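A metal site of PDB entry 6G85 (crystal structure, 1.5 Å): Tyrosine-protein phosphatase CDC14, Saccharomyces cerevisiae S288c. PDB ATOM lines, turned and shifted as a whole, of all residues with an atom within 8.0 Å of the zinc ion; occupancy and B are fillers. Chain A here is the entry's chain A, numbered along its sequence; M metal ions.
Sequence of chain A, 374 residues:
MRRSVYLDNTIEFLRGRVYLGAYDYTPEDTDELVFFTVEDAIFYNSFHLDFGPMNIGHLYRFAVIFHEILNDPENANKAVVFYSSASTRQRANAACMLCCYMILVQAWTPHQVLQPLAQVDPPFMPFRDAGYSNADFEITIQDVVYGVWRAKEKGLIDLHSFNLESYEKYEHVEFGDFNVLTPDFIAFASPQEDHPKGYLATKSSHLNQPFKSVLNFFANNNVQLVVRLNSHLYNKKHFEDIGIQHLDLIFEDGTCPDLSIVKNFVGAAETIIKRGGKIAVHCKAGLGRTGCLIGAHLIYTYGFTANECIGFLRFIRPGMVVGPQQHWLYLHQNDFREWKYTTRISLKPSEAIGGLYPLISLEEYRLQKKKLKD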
ATOM      1  N   GLN A 192     -20.283 -10.871  11.025  1.00  0.00           N
ATOM      2  CA  GLN A 192     -19.966 -12.293  11.082  1.00  0.00           C
ATOM      3  C   GLN A 192     -21.212 -13.100  11.402  1.00  0.00           C
ATOM      4  O   GLN A 192     -22.038 -12.672  12.204  1.00  0.00           O
ATOM      5  CB  GLN A 192     -18.915 -12.566  12.154  1.00  0.00           C
ATOM      6  CG  GLN A 192     -17.559 -12.000  11.821  1.00  0.00           C
ATOM      7  CD  GLN A 192     -16.550 -12.250  12.899  1.00  0.00           C
ATOM      8  OE1 GLN A 192     -16.333 -13.396  13.310  1.00  0.00           O
ATOM      9  NE2 GLN A 192     -15.942 -11.185  13.392  1.00  0.00           N
ATOM     10  N   GLU A 193     -21.308 -14.289  10.831  1.00  0.00           N
ATOM     11  CA  GLU A 193     -22.442 -15.136  11.208  1.00  0.00           C
ATOM     12  C   GLU A 193     -22.110 -16.601  10.967  1.00  0.00           C
ATOM     13  O   GLU A 193     -21.187 -16.927  10.233  1.00  0.00           O
ATOM     14  CB  GLU A 193     -23.651 -14.752  10.409  1.00  0.00           C
ATOM     15  CG  GLU A 193     -23.482 -15.051   8.941  1.00  0.00           C
ATOM     16  CD  GLU A 193     -24.825 -15.102   8.259  1.00  0.00           C
ATOM     17  OE1 GLU A 193     -25.746 -15.626   8.898  1.00  0.00           O
ATOM     18  OE2 GLU A 193     -24.971 -14.570   7.160  1.00  0.00           O
ATOM     19  N   ASP A 194     -22.941 -17.479  11.548  1.00  0.00           N
ATOM     20  CA  ASP A 194     -23.007 -18.893  11.151  1.00  0.00           C
ATOM     21  C   ASP A 194     -24.341 -19.089  10.420  1.00  0.00           C
ATOM     22  O   ASP A 194     -25.387 -19.277  11.066  1.00  0.00           O
ATOM     23  CB  ASP A 194     -22.890 -19.834  12.339  1.00  0.00           C
ATOM     24  CG  ASP A 194     -21.641 -19.588  13.181  1.00  0.00           C
ATOM     25  OD1 ASP A 194     -20.526 -19.534  12.628  1.00  0.00           O
ATOM     26  OD2 ASP A 194     -21.790 -19.465  14.414  1.00  0.00           O
ATOM     27  N   HIS A 195     -24.308 -19.033   9.090  1.00  0.00           N
ATOM     28  CA  HIS A 195     -25.534 -19.137   8.299  1.00  0.00           C
ATOM     29  C   HIS A 195     -26.002 -20.581   8.300  1.00  0.00           C
ATOM     30  O   HIS A 195     -25.320 -21.445   8.839  1.00  0.00           O
ATOM     31  CB  HIS A 195     -25.313 -18.641   6.856  1.00  0.00           C
ATOM     32  CG  HIS A 195     -26.589 -18.340   6.104  1.00  0.00           C
ATOM     33  ND1 HIS A 195     -27.451 -17.328   6.476  1.00  0.00           N
ATOM     34  CD2 HIS A 195     -27.144 -18.914   5.021  1.00  0.00           C
ATOM     35  CE1 HIS A 195     -28.474 -17.292   5.652  1.00  0.00           C
ATOM     36  NE2 HIS A 195     -28.324 -18.256   4.757  1.00  0.00           N
ATOM     37  N   HIS A 206     -31.438 -16.093  14.002  1.00  0.00           N
ATOM     38  CA  HIS A 206     -30.121 -16.602  14.336  1.00  0.00           C
ATOM     39  C   HIS A 206     -28.980 -15.548  14.243  1.00  0.00           C
ATOM     40  O   HIS A 206     -27.807 -15.884  14.466  1.00  0.00           O
ATOM     41  CB  HIS A 206     -29.783 -17.784  13.435  1.00  0.00           C
ATOM     42  CG  HIS A 206     -29.510 -17.388  12.014  1.00  0.00           C
ATOM     43  ND1 HIS A 206     -30.516 -17.184  11.087  1.00  0.00           N
ATOM     44  CD2 HIS A 206     -28.342 -17.177  11.350  1.00  0.00           C
ATOM     45  CE1 HIS A 206     -29.972 -16.865   9.925  1.00  0.00           C
ATOM     46  NE2 HIS A 206     -28.658 -16.852  10.058  1.00  0.00           N
ATOM     47  N   LEU A 207     -29.328 -14.292  13.918  1.00  0.00           N
ATOM     48  CA  LEU A 207     -28.308 -13.248  13.823  1.00  0.00           C
ATOM     49  C   LEU A 207     -27.819 -12.820  15.201  1.00  0.00           C
ATOM     50  O   LEU A 207     -28.603 -12.778  16.163  1.00  0.00           O
ATOM     51  CB  LEU A 207     -28.856 -12.043  13.056  1.00  0.00           C
ATOM     52  CG  LEU A 207     -28.889 -12.266  11.548  1.00  0.00           C
ATOM     53  CD1 LEU A 207     -29.133 -10.997  10.842  1.00  0.00           C
ATOM     54  CD2 LEU A 207     -27.570 -12.879  11.039  1.00  0.00           C
ATOM     55  N   ASN A 208     -26.519 -12.528  15.318  1.00  0.00           N
ATOM     56  CA  ASN A 208     -25.958 -12.101  16.607  1.00  0.00           C
ATOM     57  C   ASN A 208     -26.270 -10.623  16.882  1.00  0.00           C
ATOM     58  O   ASN A 208     -26.753  -9.896  16.018  1.00  0.00           O
ATOM     59  CB  ASN A 208     -24.451 -12.392  16.691  1.00  0.00           C
ATOM     60  CG  ASN A 208     -23.614 -11.735  15.541  1.00  0.00           C
ATOM     61  OD1 ASN A 208     -23.895 -10.626  15.085  1.00  0.00           O
ATOM     62  ND2 ASN A 208     -22.556 -12.449  15.109  1.00  0.00           N
ATOM     63  N   PHE A 211     -24.709  -7.831  14.506  1.00  0.00           N
ATOM     64  CA  PHE A 211     -25.296  -7.777  13.154  1.00  0.00           C
ATOM     65  C   PHE A 211     -26.690  -7.162  13.208  1.00  0.00           C
ATOM     66  O   PHE A 211     -27.036  -6.311  12.379  1.00  0.00           O
ATOM     67  CB  PHE A 211     -25.381  -9.194  12.548  1.00  0.00           C
ATOM     68  CG  PHE A 211     -25.280  -9.279  10.988  1.00  0.00           C
ATOM     69  CD1 PHE A 211     -25.503  -8.182  10.146  1.00  0.00           C
ATOM     70  CD2 PHE A 211     -24.978 -10.529  10.393  1.00  0.00           C
ATOM     71  CE1 PHE A 211     -25.433  -8.300   8.744  1.00  0.00           C
ATOM     72  CE2 PHE A 211     -24.897 -10.667   8.983  1.00  0.00           C
ATOM     73  CZ  PHE A 211     -25.117  -9.531   8.148  1.00  0.00           C
ATOM     74  N   LEU A 233     -17.502 -13.339   5.247  1.00  0.00           N
ATOM     75  CA  LEU A 233     -17.741 -13.839   6.604  1.00  0.00           C
ATOM     76  C   LEU A 233     -19.235 -13.894   6.937  1.00  0.00           C
ATOM     77  O   LEU A 233     -19.597 -14.236   8.080  1.00  0.00           O
ATOM     78  CB  LEU A 233     -17.014 -13.013   7.665  1.00  0.00           C
ATOM     79  CG  LEU A 233     -15.488 -12.800   7.466  1.00  0.00           C
ATOM     80  CD1 LEU A 233     -14.914 -11.799   8.412  1.00  0.00           C
ATOM     81  CD2 LEU A 233     -14.671 -14.130   7.555  1.00  0.00           C
ATOM     82  N   TYR A 234     -20.110 -13.614   5.969  1.00  0.00           N
ATOM     83  CA  TYR A 234     -21.542 -13.565   6.200  1.00  0.00           C
ATOM     84  C   TYR A 234     -22.240 -13.653   4.846  1.00  0.00           C
ATOM     85  O   TYR A 234     -21.611 -13.453   3.798  1.00  0.00           O
ATOM     86  CB  TYR A 234     -21.949 -12.260   6.952  1.00  0.00           C
ATOM     87  CG  TYR A 234     -21.709 -11.003   6.124  1.00  0.00           C
ATOM     88  CD1 TYR A 234     -20.500 -10.318   6.192  1.00  0.00           C
ATOM     89  CD2 TYR A 234     -22.692 -10.540   5.217  1.00  0.00           C
ATOM     90  CE1 TYR A 234     -20.277  -9.152   5.367  1.00  0.00           C
ATOM     91  CE2 TYR A 234     -22.482  -9.435   4.400  1.00  0.00           C
ATOM     92  CZ  TYR A 234     -21.275  -8.735   4.503  1.00  0.00           C
ATOM     93  OH  TYR A 234     -21.046  -7.637   3.715  1.00  0.00           O
ATOM     94  N   ASN A 235     -23.547 -13.938   4.871  1.00  0.00           N
ATOM     95  CA  ASN A 235     -24.380 -14.010   3.678  1.00  0.00           C
ATOM     96  C   ASN A 235     -24.969 -12.633   3.368  1.00  0.00           C
ATOM     97  O   ASN A 235     -25.735 -12.080   4.181  1.00  0.00           O
ATOM     98  CB  ASN A 235     -25.486 -15.072   3.864  1.00  0.00           C
ATOM     99  CG  ASN A 235     -26.225 -15.375   2.598  1.00  0.00           C
ATOM    100  OD1 ASN A 235     -26.642 -14.464   1.876  1.00  0.00           O
ATOM    101  ND2 ASN A 235     -26.402 -16.662   2.298  1.00  0.00           N
ATOM    102  N   LYS A 236     -24.651 -12.086   2.176  1.00  0.00           N
ATOM    103  CA  LYS A 236     -25.118 -10.755   1.772  1.00  0.00           C
ATOM    104  C   LYS A 236     -26.640 -10.614   1.741  1.00  0.00           C
ATOM    105  O   LYS A 236     -27.132  -9.492   1.743  1.00  0.00           O
ATOM    106  CB  LYS A 236     -24.545 -10.382   0.388  1.00  0.00           C
ATOM    107  CG  LYS A 236     -25.202 -11.188  -0.772  1.00  0.00           C
ATOM    108  CD  LYS A 236     -24.696 -10.809  -2.153  1.00  0.00           C
ATOM    109  CE  LYS A 236     -25.138 -11.770  -3.233  1.00  0.00           C
ATOM    110  NZ  LYS A 236     -26.559 -11.633  -3.595  1.00  0.00           N
ATOM    111  N   LYS A 237     -27.397 -11.720   1.695  1.00  0.00           N
ATOM    112  CA  LYS A 237     -28.854 -11.621   1.577  1.00  0.00           C
ATOM    113  C   LYS A 237     -29.481 -10.809   2.720  1.00  0.00           C
ATOM    114  O   LYS A 237     -30.535 -10.195   2.531  1.00  0.00           O
ATOM    115  CB  LYS A 237     -29.462 -13.031   1.506  1.00  0.00           C
ATOM    116  CG  LYS A 237     -30.901 -13.087   0.967  1.00  0.00           C
ATOM    117  CD  LYS A 237     -31.291 -14.499   0.553  1.00  0.00           C
ATOM    118  CE  LYS A 237     -32.808 -14.606   0.293  1.00  0.00           C
ATOM    119  NZ  LYS A 237     -33.618 -14.384   1.532  1.00  0.00           N
ATOM    120  N   HIS A 238     -28.844 -10.768   3.896  1.00  0.00           N
ATOM    121  CA  HIS A 238     -29.424 -10.030   5.029  1.00  0.00           C
ATOM    122  C   HIS A 238     -29.573  -8.549   4.713  1.00  0.00           C
ATOM    123  O   HIS A 238     -30.539  -7.903   5.136  1.00  0.00           O
ATOM    124  CB  HIS A 238     -28.582 -10.226   6.303  1.00  0.00           C
ATOM    125  CG  HIS A 238     -28.631 -11.622   6.825  1.00  0.00           C
ATOM    126  ND1 HIS A 238     -29.788 -12.199   7.304  1.00  0.00           N
ATOM    127  CD2 HIS A 238     -27.676 -12.577   6.914  1.00  0.00           C
ATOM    128  CE1 HIS A 238     -29.545 -13.443   7.670  1.00  0.00           C
ATOM    129  NE2 HIS A 238     -28.274 -13.699   7.427  1.00  0.00           N
HETATM  130 ZN    ZN M   1     -27.411 -15.707   8.084  1.00  0.00          ZN
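The side-chain carboxylate of Glu 193 sits close to a ring nitrogen (NE2) of His 206, at 3.4 Å. The backbone NH (N) of Asn 235 is in hydrogen-bond range of the side-chain carboxylate (OE2) of Glu 193 (2.8 Å). N of Glu 193 sits at hydrogen-bond distance from O of Leu 233 (3.2 Å).
Four residues have an atom within 4 Å of the zinc ion: Glu 193, His 195, His 206 and His 238. The nearest printed residue that does not touch the zinc ion is Leu 207 (4.1 Å).
The zinc ion is bound by OE1 of Glu 193. The zinc ion is bound by NE2 of His 238 (2.3 Å). The zinc ion is bound by ND1 of His 195, 2.3 Å away. The zinc ion has three donor atoms within binding distance. Slightly farther from the zinc ion lies a ring nitrogen (NE2) of His 206 (2.6 Å). Slightly farther from the zinc ion lies OE2 of Glu 193 (2.8 Å).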
